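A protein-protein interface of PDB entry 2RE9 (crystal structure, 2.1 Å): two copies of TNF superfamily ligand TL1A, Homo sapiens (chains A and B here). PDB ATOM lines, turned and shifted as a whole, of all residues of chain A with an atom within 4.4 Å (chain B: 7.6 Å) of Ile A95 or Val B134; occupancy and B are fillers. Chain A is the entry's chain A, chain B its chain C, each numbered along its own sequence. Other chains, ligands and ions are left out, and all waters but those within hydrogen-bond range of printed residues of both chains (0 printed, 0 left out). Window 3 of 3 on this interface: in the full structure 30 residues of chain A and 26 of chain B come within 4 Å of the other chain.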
ATOM      1  N   CYS A  92       6.991  22.250   4.092  1.00  0.00           N
ATOM      2  CA  CYS A  92       7.098  20.872   3.624  1.00  0.00           C
ATOM      3  C   CYS A  92       6.156  19.945   4.390  1.00  0.00           C
ATOM      4  O   CYS A  92       5.463  19.119   3.793  1.00  0.00           O
ATOM      5  CB  CYS A  92       8.535  20.355   3.764  1.00  0.00           C
ATOM      6  SG  CYS A  92       8.693  18.611   3.251  1.00  0.00           S
ATOM      7  N   SER A  93       6.139  20.083   5.711  1.00  0.00           N
ATOM      8  CA  SER A  93       5.288  19.256   6.560  1.00  0.00           C
ATOM      9  C   SER A  93       3.811  19.404   6.209  1.00  0.00           C
ATOM     10  O   SER A  93       3.095  18.411   6.078  1.00  0.00           O
ATOM     11  CB  SER A  93       5.503  19.616   8.031  1.00  0.00           C
ATOM     12  OG  SER A  93       5.215  20.984   8.270  1.00  0.00           O
ATOM     13  N   GLU A  94       3.359  20.645   6.062  1.00  0.00           N
ATOM     14  CA  GLU A  94       1.966  20.920   5.725  1.00  0.00           C
ATOM     15  C   GLU A  94       1.690  20.561   4.266  1.00  0.00           C
ATOM     16  O   GLU A  94       1.630  21.436   3.398  1.00  0.00           O
ATOM     17  CB  GLU A  94       1.647  22.399   5.965  1.00  0.00           C
ATOM     18  CG  GLU A  94       1.961  22.883   7.375  1.00  0.00           C
ATOM     19  CD  GLU A  94       1.243  22.082   8.446  1.00  0.00           C
ATOM     20  OE1 GLU A  94      -0.006  22.078   8.455  1.00  0.00           O
ATOM     21  OE2 GLU A  94       1.931  21.457   9.281  1.00  0.00           O
ATOM     22  N   ILE A  95       1.520  19.267   4.006  1.00  0.00           N
ATOM     23  CA  ILE A  95       1.259  18.770   2.660  1.00  0.00           C
ATOM     24  C   ILE A  95      -0.163  19.067   2.197  1.00  0.00           C
ATOM     25  O   ILE A  95      -1.125  18.833   2.932  1.00  0.00           O
ATOM     26  CB  ILE A  95       1.488  17.244   2.581  1.00  0.00           C
ATOM     27  CG1 ILE A  95       0.603  16.531   3.609  1.00  0.00           C
ATOM     28  CG2 ILE A  95       2.956  16.925   2.821  1.00  0.00           C
ATOM     29  CD1 ILE A  95       0.696  15.020   3.561  1.00  0.00           C
ATOM     30  N   ARG A  96      -0.290  19.582   0.977  1.00  0.00           N
ATOM     31  CA  ARG A  96      -1.596  19.903   0.412  1.00  0.00           C
ATOM     32  C   ARG A  96      -2.520  18.696   0.519  1.00  0.00           C
ATOM     33  O   ARG A  96      -2.253  17.648  -0.072  1.00  0.00           O
ATOM     34  CB  ARG A  96      -1.460  20.311  -1.056  1.00  0.00           C
ATOM     35  CG  ARG A  96      -0.718  21.617  -1.281  1.00  0.00           C
ATOM     36  CD  ARG A  96      -0.690  21.977  -2.760  1.00  0.00           C
ATOM     37  NE  ARG A  96      -0.055  23.271  -3.004  1.00  0.00           N
ATOM     38  CZ  ARG A  96       1.209  23.555  -2.705  1.00  0.00           C
ATOM     39  NH1 ARG A  96       1.984  22.636  -2.146  1.00  0.00           N
ATOM     40  NH2 ARG A  96       1.698  24.759  -2.965  1.00  0.00           N
ATOM     41  N   GLN A  97      -3.603  18.851   1.278  1.00  0.00           N
ATOM     42  CA  GLN A  97      -4.571  17.778   1.479  1.00  0.00           C
ATOM     43  C   GLN A  97      -4.990  17.141   0.157  1.00  0.00           C
ATOM     44  O   GLN A  97      -5.902  17.623  -0.516  1.00  0.00           O
ATOM     45  CB  GLN A  97      -5.808  18.314   2.208  1.00  0.00           C
ATOM     46  CG  GLN A  97      -6.849  17.252   2.533  1.00  0.00           C
ATOM     47  CD  GLN A  97      -8.051  17.811   3.272  1.00  0.00           C
ATOM     48  OE1 GLN A  97      -8.973  17.076   3.626  1.00  0.00           O
ATOM     49  NE2 GLN A  97      -8.048  19.120   3.508  1.00  0.00           N
ATOM     50  N   ARG A 100      -0.737  13.555  -1.077  1.00  0.00           N
ATOM     51  CA  ARG A 100       0.486  13.749  -1.849  1.00  0.00           C
ATOM     52  C   ARG A 100       1.486  14.634  -1.104  1.00  0.00           C
ATOM     53  O   ARG A 100       1.309  15.850  -1.009  1.00  0.00           O
ATOM     54  CB  ARG A 100       0.140  14.361  -3.214  1.00  0.00           C
ATOM     55  CG  ARG A 100       1.336  14.729  -4.085  1.00  0.00           C
ATOM     56  CD  ARG A 100       1.823  16.142  -3.798  1.00  0.00           C
ATOM     57  NE  ARG A 100       2.949  16.523  -4.645  1.00  0.00           N
ATOM     58  CZ  ARG A 100       3.522  17.722  -4.627  1.00  0.00           C
ATOM     59  NH1 ARG A 100       4.544  17.982  -5.432  1.00  0.00           N
ATOM     60  NH2 ARG A 100       3.074  18.661  -3.805  1.00  0.00           N
ATOM     61  N   PRO A 101       2.547  14.024  -0.548  1.00  0.00           N
ATOM     62  CA  PRO A 101       3.579  14.760   0.191  1.00  0.00           C
ATOM     63  C   PRO A 101       4.400  15.659  -0.731  1.00  0.00           C
ATOM     64  O   PRO A 101       4.510  15.399  -1.929  1.00  0.00           O
ATOM     65  CB  PRO A 101       4.423  13.646   0.808  1.00  0.00           C
ATOM     66  CG  PRO A 101       3.444  12.522   0.962  1.00  0.00           C
ATOM     67  CD  PRO A 101       2.708  12.574  -0.350  1.00  0.00           C
ATOM     68  N   ASN A 102       4.979  16.712  -0.166  1.00  0.00           N
ATOM     69  CA  ASN A 102       5.786  17.648  -0.938  1.00  0.00           C
ATOM     70  C   ASN A 102       7.253  17.240  -0.924  1.00  0.00           C
ATOM     71  O   ASN A 102       7.688  16.495  -0.047  1.00  0.00           O
ATOM     72  CB  ASN A 102       5.657  19.053  -0.353  1.00  0.00           C
ATOM     73  CG  ASN A 102       4.217  19.489  -0.201  1.00  0.00           C
ATOM     74  OD1 ASN A 102       3.480  19.590  -1.182  1.00  0.00           O
ATOM     75  ND2 ASN A 102       3.805  19.747   1.035  1.00  0.00           N
ATOM     76  N   CYS A 132      12.324  18.125   6.479  1.00  0.00           N
ATOM     77  CA  CYS A 132      10.889  18.352   6.378  1.00  0.00           C
ATOM     78  C   CYS A 132      10.397  18.280   7.820  1.00  0.00           C
ATOM     79  O   CYS A 132       9.862  17.266   8.262  1.00  0.00           O
ATOM     80  CB  CYS A 132      10.246  17.259   5.519  1.00  0.00           C
ATOM     81  SG  CYS A 132       8.522  17.545   4.978  1.00  0.00           S
ATOM     82  N   VAL A 134       8.277  19.466  11.379  1.00  0.00           N
ATOM     83  CA  VAL A 134       6.890  19.730  11.737  1.00  0.00           C
ATOM     84  C   VAL A 134       6.812  20.691  12.920  1.00  0.00           C
ATOM     85  O   VAL A 134       5.754  21.245  13.206  1.00  0.00           O
ATOM     86  CB  VAL A 134       6.133  18.426  12.095  1.00  0.00           C
ATOM     87  CG1 VAL A 134       6.103  17.497  10.894  1.00  0.00           C
ATOM     88  CG2 VAL A 134       6.792  17.743  13.273  1.00  0.00           C
ATOM     89  N   THR B  89       9.365   7.930   1.110  1.00  0.00           N
ATOM     90  CA  THR B  89       8.733   7.974   2.422  1.00  0.00           C
ATOM     91  C   THR B  89       7.631   6.938   2.601  1.00  0.00           C
ATOM     92  O   THR B  89       6.668   6.905   1.837  1.00  0.00           O
ATOM     93  CB  THR B  89       8.134   9.358   2.697  1.00  0.00           C
ATOM     94  OG1 THR B  89       9.184  10.328   2.750  1.00  0.00           O
ATOM     95  CG2 THR B  89       7.379   9.358   4.016  1.00  0.00           C
ATOM     96  N   SER B  90       7.776   6.102   3.623  1.00  0.00           N
ATOM     97  CA  SER B  90       6.780   5.077   3.908  1.00  0.00           C
ATOM     98  C   SER B  90       5.520   5.761   4.419  1.00  0.00           C
ATOM     99  O   SER B  90       5.387   6.981   4.333  1.00  0.00           O
ATOM    100  CB  SER B  90       7.297   4.104   4.972  1.00  0.00           C
ATOM    101  OG  SER B  90       7.408   4.740   6.233  1.00  0.00           O
ATOM    102  N   CYS B  92       4.604   5.678   7.564  1.00  0.00           N
ATOM    103  CA  CYS B  92       4.758   5.808   9.008  1.00  0.00           C
ATOM    104  C   CYS B  92       3.991   7.028   9.496  1.00  0.00           C
ATOM    105  O   CYS B  92       3.420   7.021  10.587  1.00  0.00           O
ATOM    106  CB  CYS B  92       6.236   5.954   9.391  1.00  0.00           C
ATOM    107  SG  CYS B  92       6.483   6.309  11.164  1.00  0.00           S
ATOM    108  N   SER B  93       3.980   8.074   8.676  1.00  0.00           N
ATOM    109  CA  SER B  93       3.286   9.311   9.012  1.00  0.00           C
ATOM    110  C   SER B  93       2.006   9.464   8.195  1.00  0.00           C
ATOM    111  O   SER B  93       2.046   9.859   7.030  1.00  0.00           O
ATOM    112  CB  SER B  93       4.205  10.507   8.759  1.00  0.00           C
ATOM    113  OG  SER B  93       4.654  10.525   7.415  1.00  0.00           O
ATOM    114  N   GLU B  94       0.872   9.150   8.814  1.00  0.00           N
ATOM    115  CA  GLU B  94      -0.420   9.254   8.144  1.00  0.00           C
ATOM    116  C   GLU B  94      -1.524   9.659   9.117  1.00  0.00           C
ATOM    117  O   GLU B  94      -1.309  10.482  10.010  1.00  0.00           O
ATOM    118  CB  GLU B  94      -0.782   7.919   7.485  1.00  0.00           C
ATOM    119  CG  GLU B  94       0.183   7.471   6.400  1.00  0.00           C
ATOM    120  CD  GLU B  94       0.236   8.430   5.226  1.00  0.00           C
ATOM    121  OE1 GLU B  94       1.015   8.172   4.285  1.00  0.00           O
ATOM    122  OE2 GLU B  94      -0.501   9.439   5.242  1.00  0.00           O
ATOM    123  N   CYS B 132      10.970   8.206   9.947  1.00  0.00           N
ATOM    124  CA  CYS B 132       9.533   8.413   9.834  1.00  0.00           C
ATOM    125  C   CYS B 132       9.269   9.833   9.342  1.00  0.00           C
ATOM    126  O   CYS B 132       8.617  10.617  10.027  1.00  0.00           O
ATOM    127  CB  CYS B 132       8.871   8.195  11.197  1.00  0.00           C
ATOM    128  SG  CYS B 132       7.047   8.260  11.223  1.00  0.00           S
ATOM    129  N   GLU B 133       9.781  10.158   8.155  1.00  0.00           N
ATOM    130  CA  GLU B 133       9.604  11.493   7.592  1.00  0.00           C
ATOM    131  C   GLU B 133       8.236  11.691   6.955  1.00  0.00           C
ATOM    132  O   GLU B 133       7.581  10.729   6.561  1.00  0.00           O
ATOM    133  CB  GLU B 133      10.704  11.793   6.569  1.00  0.00           C
ATOM    134  CG  GLU B 133      12.095  11.908   7.175  1.00  0.00           C
ATOM    135  CD  GLU B 133      13.058  12.685   6.290  1.00  0.00           C
ATOM    136  OE1 GLU B 133      14.255  12.779   6.645  1.00  0.00           O
ATOM    137  OE2 GLU B 133      12.618  13.207   5.241  1.00  0.00           O
ATOM    138  N   VAL B 134       7.813  12.947   6.852  1.00  0.00           N
ATOM    139  CA  VAL B 134       6.508  13.274   6.287  1.00  0.00           C
ATOM    140  C   VAL B 134       6.574  13.902   4.903  1.00  0.00           C
ATOM    141  O   VAL B 134       5.613  14.526   4.461  1.00  0.00           O
ATOM    142  CB  VAL B 134       5.736  14.246   7.204  1.00  0.00           C
ATOM    143  CG1 VAL B 134       5.665  13.689   8.615  1.00  0.00           C
ATOM    144  CG2 VAL B 134       6.407  15.609   7.198  1.00  0.00           C
ATOM    145  N   GLY B 135       7.697  13.740   4.217  1.00  0.00           N
ATOM    146  CA  GLY B 135       7.819  14.325   2.896  1.00  0.00           C
ATOM    147  C   GLY B 135       7.768  13.305   1.780  1.00  0.00           C
ATOM    148  O   GLY B 135       7.591  12.115   2.023  1.00  0.00           O
ATOM    149  N   SER B 136       7.917  13.783   0.549  1.00  0.00           N
ATOM    150  CA  SER B 136       7.908  12.928  -0.630  1.00  0.00           C
ATOM    151  C   SER B 136       8.920  11.804  -0.470  1.00  0.00           C
ATOM    152  O   SER B 136       8.583  10.625  -0.589  1.00  0.00           O
ATOM    153  CB  SER B 136       8.255  13.755  -1.867  1.00  0.00           C
ATOM    154  OG  SER B 136       8.688  12.923  -2.928  1.00  0.00           O
ATOM    155  N   ASN B 137      10.166  12.182  -0.210  1.00  0.00           N
ATOM    156  CA  ASN B 137      11.240  11.217  -0.025  1.00  0.00           C
ATOM    157  C   ASN B 137      12.185  11.722   1.056  1.00  0.00           C
ATOM    158  O   ASN B 137      11.959  12.780   1.647  1.00  0.00           O
ATOM    159  CB  ASN B 137      11.998  10.999  -1.339  1.00  0.00           C
ATOM    160  CG  ASN B 137      12.575  12.281  -1.901  1.00  0.00           C
ATOM    161  OD1 ASN B 137      11.843  13.227  -2.196  1.00  0.00           O
ATOM    162  ND2 ASN B 137      13.896  12.321  -2.058  1.00  0.00           N
ATOM    163  N   TRP B 138      13.242  10.962   1.318  1.00  0.00           N
ATOM    164  CA  TRP B 138      14.196  11.333   2.348  1.00  0.00           C
ATOM    165  C   TRP B 138      15.574  10.754   2.080  1.00  0.00           C
ATOM    166  O   TRP B 138      15.736   9.816   1.303  1.00  0.00           O
ATOM    167  CB  TRP B 138      13.719  10.825   3.708  1.00  0.00           C
ATOM    168  CG  TRP B 138      13.533   9.331   3.725  1.00  0.00           C
ATOM    169  CD1 TRP B 138      12.395   8.641   3.412  1.00  0.00           C
ATOM    170  CD2 TRP B 138      14.534   8.343   4.012  1.00  0.00           C
ATOM    171  NE1 TRP B 138      12.626   7.287   3.485  1.00  0.00           N
ATOM    172  CE2 TRP B 138      13.929   7.075   3.850  1.00  0.00           C
ATOM    173  CE3 TRP B 138      15.884   8.405   4.387  1.00  0.00           C
ATOM    174  CZ2 TRP B 138      14.625   5.878   4.050  1.00  0.00           C
ATOM    175  CZ3 TRP B 138      16.578   7.213   4.587  1.00  0.00           C
ATOM    176  CH2 TRP B 138      15.943   5.965   4.417  1.00  0.00           C
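The backbone NH of Ser B136 is in hydrogen-bond range of the backbone carbonyl oxygen of Asn A102.
The backbone carbonyl oxygen of Cys A92 is in hydrogen-bond range of the side-chain amide nitrogen of Asn A102, 3.3 Å away. SG of Cys A92 forms a disulfide with SG of Cys A132 (2.0 Å). OE2 of Glu A94 lies within hydrogen-bond range of OG of Ser A93. The side-chain hydroxyl (OG1) of Thr B89 lies within hydrogen-bond range of the backbone carbonyl oxygen (O) of Gly B135 (2.5 Å). The backbone carbonyl oxygen (O) of Ser B136 sits at hydrogen-bond distance from the backbone NH (N) of Thr B89 (3.3 Å). The side-chain hydroxyl (OG) of Ser B136 lies within hydrogen-bond range of the side-chain amide oxygen (OD1) of Asn B137, at 3.3 Å.
Among the printed residues, pairs that only touch across the chains: Pro A101 with Gly B135, Pro A101 with Ser B136, Cys A132 with Val B134, Asn A102 with Gly B135, Ser A93 with Val B134, Cys A132 with Gly B135, Ile A95 with Val B134 and Pro A101 with Val B134.
Cys A92 touches none of the printed residues of chain B. Of chain B, only Val B134 comes within 4 Å of Ile A95. Arg A96 touches none of the printed residues of chain B. Of the printed residues of chain B, Cys A132 touches Val B134 and Gly B135. Printed residues of chain A within 4 Å of Gly B135: Pro A101, Asn A102 and Cys A132. The nearest printed residue of chain B that does not touch Asn A102 is Asn B137 (5.0 Å).
Of the 12 printed residues of chain B, 3 touch a printed residue of chain A. Hydrophobic or aromatic side chains of chain A that line the printed part of chain B: Ile A95 and Pro A101. Among the printed residues, 9 pairs touch across the chains.
Ser A93 touches Val B134, but with the chains exchanged Val A134 does not touch Ser B93 (7.6 Å). Cys A132 touches Val B134, but with the chains exchanged Val A134 does not touch Cys B132 (7.4 Å). 5 positions are printed for both chains. Of the 9 pairs that touch across the chains among the printed residues, none has its exchanged pair printed and touching as well.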
